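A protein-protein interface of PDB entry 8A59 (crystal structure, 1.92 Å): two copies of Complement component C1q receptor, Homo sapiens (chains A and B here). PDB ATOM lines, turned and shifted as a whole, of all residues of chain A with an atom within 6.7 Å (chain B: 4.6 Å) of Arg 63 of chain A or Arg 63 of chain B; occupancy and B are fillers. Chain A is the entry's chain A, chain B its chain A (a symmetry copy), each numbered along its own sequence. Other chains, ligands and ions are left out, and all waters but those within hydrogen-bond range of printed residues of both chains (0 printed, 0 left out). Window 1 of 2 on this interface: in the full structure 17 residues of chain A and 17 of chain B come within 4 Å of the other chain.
Arg 56 of chain A touches Arg 63 of chain B (CD to NH2, 3.4 Å). O of Leu 62 of chain A touches CB of Ser 193 of chain B (3.9 Å). NH2 of Arg 63 of chain A touches CD of Arg 56 of chain B, 3.4 Å away. NH2 of Arg 64 of chain B touches NE of Arg 64 of chain A (3.6 Å). Ser 193 of chain A touches Leu 62 of chain B (CB to O, 3.9 Å).
Printed residues of chain A that touch a printed residue of chain B: Arg 56, Gln 60, Leu 62, Arg 63, Arg 64 and Ser 193. Among the printed residues, 8 pairs touch across the chains. Among the printed residues, no Asp or Glu carboxylate lies within 4 Å of a Lys or Arg side-chain nitrogen of the other chain.
The guanidinium group (NH1) of Arg 56 of chain A is in salt-bridge range of the side-chain carboxylate (OE2) of Glu 195 of chain A, 2.8 Å away. The backbone NH of Val 11 of chain A is in hydrogen-bond range of the side-chain amide oxygen of Gln 60 of chain A (3.2 Å).
Arg 56 of chain A touches Arg 63 of chain B, and with the chains exchanged Arg 63 of chain A touches Arg 56 of chain B. Leu 62 of chain A touches Ser 193 of chain B, and with the chains exchanged Ser 193 of chain A touches Leu 62 of chain B. Arg 63 of chain B touches its own counterpart, Arg 63 of chain A. Arg 64 of chain B touches its own counterpart, Arg 64 of chain A. Positions printed for both chains: 56, 59, 60, 61, 62, 63, 64, 65 and 193. Of the 8 pairs that touch across the chains among the printed residues, 8 have their exchanged pair printed and touching as well.
Arg 63 of chain A touches just these residues of chain B: Arg 56, Gln 60 and Arg 63. Of the printed residues of chain A, Gln 60 of chain B touches Arg 63. Of the printed residues of chain A, Leu 62 of chain B touches Ser 193 (3.9 Å). Printed residues of chain A within 4 Å of Arg 64 of chain B: Arg 64 (3.6 Å). Leu 61 of chain B touches none of the printed residues of chain A. Glu 195 of chain A touches none of the printed residues of chain B. The nearest printed residue of chain A that does not touch Arg 56 of chain B is Ala 59 of chain A (6.2 Å).
The guanidinium group (NE) of Arg 63 of chain B lies close to the side-chain amide nitrogen (NE2) of Gln 60 of chain A (2.7 Å). NE2 of Gln 60 of chain B lies close to NE of Arg 63 of chain A, at 2.7 Å. The guanidinium group of Arg 63 of chain A sits close to the guanidinium group of Arg 63 of chain B, at 3.4 Å.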
ATOM      1  N   GLU A   9       4.176 -33.699  37.320  1.00  0.00           N
ATOM      2  CA  GLU A   9       3.863 -34.109  35.958  1.00  0.00           C
ATOM      3  C   GLU A   9       4.531 -33.146  34.983  1.00  0.00           C
ATOM      4  O   GLU A   9       4.421 -33.317  33.767  1.00  0.00           O
ATOM      5  CB  GLU A   9       2.353 -34.079  35.709  1.00  0.00           C
ATOM      6  CG  GLU A   9       1.534 -34.445  36.930  1.00  0.00           C
ATOM      7  CD  GLU A   9       0.060 -34.648  36.627  1.00  0.00           C
ATOM      8  OE1 GLU A   9      -0.724 -33.735  36.931  1.00  0.00           O
ATOM      9  OE2 GLU A   9      -0.294 -35.721  36.094  1.00  0.00           O
ATOM     10  N   VAL A  11       7.454 -31.935  33.154  1.00  0.00           N
ATOM     11  CA  VAL A  11       8.767 -32.390  32.722  1.00  0.00           C
ATOM     12  C   VAL A  11       8.905 -32.089  31.240  1.00  0.00           C
ATOM     13  O   VAL A  11       7.954 -32.217  30.465  1.00  0.00           O
ATOM     14  CB  VAL A  11       9.012 -33.882  33.053  1.00  0.00           C
ATOM     15  CG1 VAL A  11       7.920 -34.746  32.441  1.00  0.00           C
ATOM     16  CG2 VAL A  11      10.399 -34.342  32.589  1.00  0.00           C
ATOM     17  N   VAL A  12      10.099 -31.615  30.873  1.00  0.00           N
ATOM     18  CA  VAL A  12      10.511 -31.477  29.491  1.00  0.00           C
ATOM     19  C   VAL A  12      11.908 -32.112  29.421  1.00  0.00           C
ATOM     20  O   VAL A  12      12.709 -31.885  30.323  1.00  0.00           O
ATOM     21  CB  VAL A  12      10.535 -29.977  29.132  1.00  0.00           C
ATOM     22  CG1 VAL A  12      11.212 -29.698  27.801  1.00  0.00           C
ATOM     23  CG2 VAL A  12       9.146 -29.330  29.174  1.00  0.00           C
ATOM     24  N   ARG A  56       8.702 -23.366  29.625  1.00  0.00           N
ATOM     25  CA  ARG A  56       7.792 -24.401  29.170  1.00  0.00           C
ATOM     26  C   ARG A  56       7.441 -25.353  30.302  1.00  0.00           C
ATOM     27  O   ARG A  56       6.283 -25.708  30.478  1.00  0.00           O
ATOM     28  CB  ARG A  56       8.359 -25.134  27.938  1.00  0.00           C
ATOM     29  CG  ARG A  56       7.311 -25.896  27.133  1.00  0.00           C
ATOM     30  CD  ARG A  56       7.762 -27.017  26.191  1.00  0.00           C
ATOM     31  NE  ARG A  56       9.089 -26.750  25.655  1.00  0.00           N
ATOM     32  CZ  ARG A  56       9.869 -27.657  25.056  1.00  0.00           C
ATOM     33  NH1 ARG A  56       9.437 -28.895  24.847  1.00  0.00           N
ATOM     34  NH2 ARG A  56      11.084 -27.311  24.658  1.00  0.00           N
ATOM     35  N   VAL A  57       8.428 -25.740  31.115  1.00  0.00           N
ATOM     36  CA  VAL A  57       8.067 -26.629  32.193  1.00  0.00           C
ATOM     37  C   VAL A  57       7.237 -25.899  33.261  1.00  0.00           C
ATOM     38  O   VAL A  57       6.350 -26.496  33.893  1.00  0.00           O
ATOM     39  CB  VAL A  57       9.289 -27.376  32.752  1.00  0.00           C
ATOM     40  CG1 VAL A  57      10.237 -26.475  33.548  1.00  0.00           C
ATOM     41  CG2 VAL A  57       8.881 -28.600  33.562  1.00  0.00           C
ATOM     42  N   LEU A  58       7.531 -24.622  33.512  1.00  0.00           N
ATOM     43  CA  LEU A  58       6.688 -23.906  34.471  1.00  0.00           C
ATOM     44  C   LEU A  58       5.236 -23.780  33.984  1.00  0.00           C
ATOM     45  O   LEU A  58       4.287 -23.861  34.788  1.00  0.00           O
ATOM     46  CB  LEU A  58       7.297 -22.534  34.741  1.00  0.00           C
ATOM     47  CG  LEU A  58       8.580 -22.534  35.588  1.00  0.00           C
ATOM     48  CD1 LEU A  58       9.277 -21.190  35.463  1.00  0.00           C
ATOM     49  CD2 LEU A  58       8.269 -22.822  37.057  1.00  0.00           C
ATOM     50  N   ALA A  59       5.059 -23.526  32.677  1.00  0.00           N
ATOM     51  CA  ALA A  59       3.727 -23.399  32.087  1.00  0.00           C
ATOM     52  C   ALA A  59       2.945 -24.691  32.293  1.00  0.00           C
ATOM     53  O   ALA A  59       1.751 -24.663  32.598  1.00  0.00           O
ATOM     54  CB  ALA A  59       3.828 -23.036  30.616  1.00  0.00           C
ATOM     55  N   GLN A  60       3.648 -25.831  32.177  1.00  0.00           N
ATOM     56  CA  GLN A  60       3.029 -27.128  32.392  1.00  0.00           C
ATOM     57  C   GLN A  60       2.609 -27.259  33.854  1.00  0.00           C
ATOM     58  O   GLN A  60       1.542 -27.790  34.151  1.00  0.00           O
ATOM     59  CB  GLN A  60       3.963 -28.303  32.047  1.00  0.00           C
ATOM     60  CG  GLN A  60       4.150 -28.560  30.561  1.00  0.00           C
ATOM     61  CD  GLN A  60       5.127 -29.703  30.365  1.00  0.00           C
ATOM     62  OE1 GLN A  60       5.285 -30.555  31.231  1.00  0.00           O
ATOM     63  NE2 GLN A  60       5.795 -29.736  29.221  1.00  0.00           N
ATOM     64  N   LEU A  61       3.493 -26.863  34.770  1.00  0.00           N
ATOM     65  CA  LEU A  61       3.139 -26.921  36.169  1.00  0.00           C
ATOM     66  C   LEU A  61       1.853 -26.118  36.415  1.00  0.00           C
ATOM     67  O   LEU A  61       0.950 -26.602  37.098  1.00  0.00           O
ATOM     68  CB  LEU A  61       4.293 -26.379  37.020  1.00  0.00           C
ATOM     69  CG  LEU A  61       4.046 -26.378  38.528  1.00  0.00           C
ATOM     70  CD1 LEU A  61       3.950 -27.801  39.075  1.00  0.00           C
ATOM     71  CD2 LEU A  61       5.146 -25.620  39.256  1.00  0.00           C
ATOM     72  N   LEU A  62       1.768 -24.893  35.878  1.00  0.00           N
ATOM     73  CA  LEU A  62       0.578 -24.085  36.143  1.00  0.00           C
ATOM     74  C   LEU A  62      -0.699 -24.738  35.606  1.00  0.00           C
ATOM     75  O   LEU A  62      -1.742 -24.615  36.235  1.00  0.00           O
ATOM     76  CB  LEU A  62       0.754 -22.681  35.580  1.00  0.00           C
ATOM     77  CG  LEU A  62       1.930 -21.927  36.179  1.00  0.00           C
ATOM     78  CD1 LEU A  62       2.217 -20.672  35.384  1.00  0.00           C
ATOM     79  CD2 LEU A  62       1.711 -21.654  37.656  1.00  0.00           C
ATOM     80  N   ARG A  63      -0.622 -25.400  34.447  1.00  0.00           N
ATOM     81  CA  ARG A  63      -1.749 -26.127  33.885  1.00  0.00           C
ATOM     82  C   ARG A  63      -2.101 -27.347  34.742  1.00  0.00           C
ATOM     83  O   ARG A  63      -3.266 -27.732  34.791  1.00  0.00           O
ATOM     84  CB  ARG A  63      -1.477 -26.583  32.450  1.00  0.00           C
ATOM     85  CG  ARG A  63      -1.674 -25.527  31.368  1.00  0.00           C
ATOM     86  CD  ARG A  63      -1.148 -26.199  30.098  1.00  0.00           C
ATOM     87  NE  ARG A  63      -0.625 -25.351  29.032  1.00  0.00           N
ATOM     88  CZ  ARG A  63       0.617 -25.354  28.537  1.00  0.00           C
ATOM     89  NH1 ARG A  63       1.542 -26.187  28.998  1.00  0.00           N
ATOM     90  NH2 ARG A  63       0.924 -24.521  27.557  1.00  0.00           N
ATOM     91  N   ARG A  64      -1.097 -27.982  35.375  1.00  0.00           N
ATOM     92  CA  ARG A  64      -1.301 -29.227  36.111  1.00  0.00           C
ATOM     93  C   ARG A  64      -1.742 -28.974  37.557  1.00  0.00           C
ATOM     94  O   ARG A  64      -2.400 -29.833  38.140  1.00  0.00           O
ATOM     95  CB  ARG A  64      -0.052 -30.123  36.149  1.00  0.00           C
ATOM     96  CG  ARG A  64       0.545 -30.504  34.796  1.00  0.00           C
ATOM     97  CD  ARG A  64      -0.185 -31.498  33.920  1.00  0.00           C
ATOM     98  NE  ARG A  64      -1.067 -30.808  32.985  1.00  0.00           N
ATOM     99  CZ  ARG A  64      -2.383 -30.980  32.900  1.00  0.00           C
ATOM    100  NH1 ARG A  64      -2.994 -31.850  33.688  1.00  0.00           N
ATOM    101  NH2 ARG A  64      -3.087 -30.284  32.025  1.00  0.00           N
ATOM    102  N   GLU A  65      -1.336 -27.849  38.163  1.00  0.00           N
ATOM    103  CA  GLU A  65      -1.607 -27.597  39.577  1.00  0.00           C
ATOM    104  C   GLU A  65      -2.531 -26.389  39.744  1.00  0.00           C
ATOM    105  O   GLU A  65      -2.073 -25.243  39.790  1.00  0.00           O
ATOM    106  CB  GLU A  65      -0.325 -27.433  40.397  1.00  0.00           C
ATOM    107  CG  GLU A  65       0.333 -28.758  40.742  1.00  0.00           C
ATOM    108  N   ALA A  66      -3.836 -26.673  39.891  1.00  0.00           N
ATOM    109  CA  ALA A  66      -4.877 -25.648  39.949  1.00  0.00           C
ATOM    110  C   ALA A  66      -4.734 -24.782  41.207  1.00  0.00           C
ATOM    111  O   ALA A  66      -5.285 -23.680  41.273  1.00  0.00           O
ATOM    112  CB  ALA A  66      -6.260 -26.283  39.840  1.00  0.00           C
ATOM    113  N   SER A 192       4.340 -38.801  29.573  1.00  0.00           N
ATOM    114  CA  SER A 192       4.253 -39.103  28.155  1.00  0.00           C
ATOM    115  C   SER A 192       4.794 -37.928  27.346  1.00  0.00           C
ATOM    116  O   SER A 192       5.044 -36.845  27.886  1.00  0.00           O
ATOM    117  CB  SER A 192       2.831 -39.430  27.749  1.00  0.00           C
ATOM    118  OG  SER A 192       2.647 -39.249  26.347  1.00  0.00           O
ATOM    119  N   SER A 193       4.985 -38.175  26.044  1.00  0.00           N
ATOM    120  CA  SER A 193       5.551 -37.200  25.133  1.00  0.00           C
ATOM    121  C   SER A 193       6.833 -36.589  25.720  1.00  0.00           C
ATOM    122  O   SER A 193       6.877 -35.399  26.016  1.00  0.00           O
ATOM    123  CB  SER A 193       4.506 -36.160  24.825  1.00  0.00           C
ATOM    124  OG  SER A 193       4.774 -35.516  23.592  1.00  0.00           O
ATOM    125  N   GLU A 195      10.675 -35.709  24.655  1.00  0.00           N
ATOM    126  CA  GLU A 195      11.312 -35.495  23.365  1.00  0.00           C
ATOM    127  C   GLU A 195      12.649 -36.249  23.322  1.00  0.00           C
ATOM    128  O   GLU A 195      13.168 -36.567  22.257  1.00  0.00           O
ATOM    129  CB  GLU A 195      11.356 -33.991  23.067  1.00  0.00           C
ATOM    130  CG  GLU A 195       9.962 -33.406  22.842  1.00  0.00           C
ATOM    131  CD  GLU A 195       9.661 -31.984  23.307  1.00  0.00           C
ATOM    132  OE1 GLU A 195       8.788 -31.329  22.676  1.00  0.00           O
ATOM    133  OE2 GLU A 195      10.268 -31.538  24.308  1.00  0.00           O
ATOM    134  N   ARG B  56       1.441 -24.103  20.578  1.00  0.00           N
ATOM    135  CA  ARG B  56       1.275 -24.339  22.000  1.00  0.00           C
ATOM    136  C   ARG B  56       0.068 -25.225  22.267  1.00  0.00           C
ATOM    137  O   ARG B  56       0.143 -26.151  23.065  1.00  0.00           O
ATOM    138  CB  ARG B  56       1.213 -23.010  22.777  1.00  0.00           C
ATOM    139  CG  ARG B  56       1.497 -23.151  24.270  1.00  0.00           C
ATOM    140  CD  ARG B  56       1.030 -22.048  25.226  1.00  0.00           C
ATOM    141  NE  ARG B  56       1.029 -20.749  24.570  1.00  0.00           N
ATOM    142  CZ  ARG B  56       0.404 -19.659  25.030  1.00  0.00           C
ATOM    143  NH1 ARG B  56      -0.229 -19.679  26.196  1.00  0.00           N
ATOM    144  NH2 ARG B  56       0.427 -18.545  24.315  1.00  0.00           N
ATOM    145  N   ALA B  59       0.977 -28.793  21.218  1.00  0.00           N
ATOM    146  CA  ALA B  59       1.901 -29.401  22.173  1.00  0.00           C
ATOM    147  C   ALA B  59       1.126 -29.947  23.367  1.00  0.00           C
ATOM    148  O   ALA B  59       1.424 -31.033  23.868  1.00  0.00           O
ATOM    149  CB  ALA B  59       2.957 -28.398  22.605  1.00  0.00           C
ATOM    150  N   GLN B  60       0.087 -29.204  23.785  1.00  0.00           N
ATOM    151  CA  GLN B  60      -0.758 -29.635  24.886  1.00  0.00           C
ATOM    152  C   GLN B  60      -1.518 -30.897  24.485  1.00  0.00           C
ATOM    153  O   GLN B  60      -1.676 -31.812  25.289  1.00  0.00           O
ATOM    154  CB  GLN B  60      -1.781 -28.566  25.312  1.00  0.00           C
ATOM    155  CG  GLN B  60      -1.206 -27.409  26.113  1.00  0.00           C
ATOM    156  CD  GLN B  60      -2.307 -26.411  26.419  1.00  0.00           C
ATOM    157  OE1 GLN B  60      -3.481 -26.758  26.466  1.00  0.00           O
ATOM    158  NE2 GLN B  60      -1.939 -25.156  26.632  1.00  0.00           N
ATOM    159  N   LEU B  61      -2.072 -30.903  23.272  1.00  0.00           N
ATOM    160  CA  LEU B  61      -2.768 -32.084  22.816  1.00  0.00           C
ATOM    161  C   LEU B  61      -1.831 -33.299  22.884  1.00  0.00           C
ATOM    162  O   LEU B  61      -2.233 -34.356  23.374  1.00  0.00           O
ATOM    163  CB  LEU B  61      -3.279 -31.867  21.388  1.00  0.00           C
ATOM    164  CG  LEU B  61      -4.032 -33.050  20.779  1.00  0.00           C
ATOM    165  CD1 LEU B  61      -5.353 -33.298  21.505  1.00  0.00           C
ATOM    166  CD2 LEU B  61      -4.295 -32.819  19.298  1.00  0.00           C
ATOM    167  N   LEU B  62      -0.594 -33.165  22.386  1.00  0.00           N
ATOM    168  CA  LEU B  62       0.299 -34.322  22.388  1.00  0.00           C
ATOM    169  C   LEU B  62       0.599 -34.824  23.803  1.00  0.00           C
ATOM    170  O   LEU B  62       0.728 -36.026  23.996  1.00  0.00           O
ATOM    171  CB  LEU B  62       1.585 -34.001  21.637  1.00  0.00           C
ATOM    172  CG  LEU B  62       1.364 -33.629  20.180  1.00  0.00           C
ATOM    173  CD1 LEU B  62       2.628 -33.052  19.581  1.00  0.00           C
ATOM    174  CD2 LEU B  62       0.818 -34.805  19.391  1.00  0.00           C
ATOM    175  N   ARG B  63       0.732 -33.913  24.773  1.00  0.00           N
ATOM    176  CA  ARG B  63       0.935 -34.278  26.166  1.00  0.00           C
ATOM    177  C   ARG B  63      -0.314 -34.947  26.748  1.00  0.00           C
ATOM    178  O   ARG B  63      -0.189 -35.789  27.633  1.00  0.00           O
ATOM    179  CB  ARG B  63       1.302 -33.067  27.027  1.00  0.00           C
ATOM    180  CG  ARG B  63       2.763 -32.631  26.972  1.00  0.00           C
ATOM    181  CD  ARG B  63       2.782 -31.315  27.752  1.00  0.00           C
ATOM    182  NE  ARG B  63       3.810 -30.333  27.424  1.00  0.00           N
ATOM    183  CZ  ARG B  63       3.619 -29.088  26.974  1.00  0.00           C
ATOM    184  NH1 ARG B  63       2.400 -28.604  26.778  1.00  0.00           N
ATOM    185  NH2 ARG B  63       4.670 -28.319  26.735  1.00  0.00           N
ATOM    186  N   ARG B  64      -1.514 -34.545  26.292  1.00  0.00           N
ATOM    187  CA  ARG B  64      -2.769 -35.022  26.867  1.00  0.00           C
ATOM    188  C   ARG B  64      -3.229 -36.339  26.231  1.00  0.00           C
ATOM    189  O   ARG B  64      -3.943 -37.098  26.881  1.00  0.00           O
ATOM    190  CB  ARG B  64      -3.920 -34.010  26.740  1.00  0.00           C
ATOM    191  CG  ARG B  64      -3.666 -32.623  27.328  1.00  0.00           C
ATOM    192  CD  ARG B  64      -3.633 -32.452  28.831  1.00  0.00           C
ATOM    193  NE  ARG B  64      -2.267 -32.572  29.331  1.00  0.00           N
ATOM    194  CZ  ARG B  64      -1.853 -33.464  30.227  1.00  0.00           C
ATOM    195  NH1 ARG B  64      -2.708 -34.325  30.756  1.00  0.00           N
ATOM    196  NH2 ARG B  64      -0.584 -33.494  30.594  1.00  0.00           N
ATOM    197  N   GLU B  65      -2.892 -36.586  24.957  1.00  0.00           N
ATOM    198  CA  GLU B  65      -3.399 -37.756  24.242  1.00  0.00           C
ATOM    199  C   GLU B  65      -2.255 -38.704  23.877  1.00  0.00           C
ATOM    200  O   GLU B  65      -1.607 -38.546  22.837  1.00  0.00           O
ATOM    201  CB  GLU B  65      -4.219 -37.375  23.007  1.00  0.00           C
ATOM    202  CG  GLU B  65      -5.637 -36.947  23.345  1.00  0.00           C
ATOM    203  N   SER B 193      -6.075 -22.555  34.254  1.00  0.00           N
ATOM    204  CA  SER B 193      -5.056 -21.660  33.742  1.00  0.00           C
ATOM    205  C   SER B 193      -5.417 -21.182  32.326  1.00  0.00           C
ATOM    206  O   SER B 193      -4.722 -21.500  31.366  1.00  0.00           O
ATOM    207  CB  SER B 193      -3.724 -22.361  33.791  1.00  0.00           C
ATOM    208  OG  SER B 193      -2.657 -21.429  33.825  1.00  0.00           O
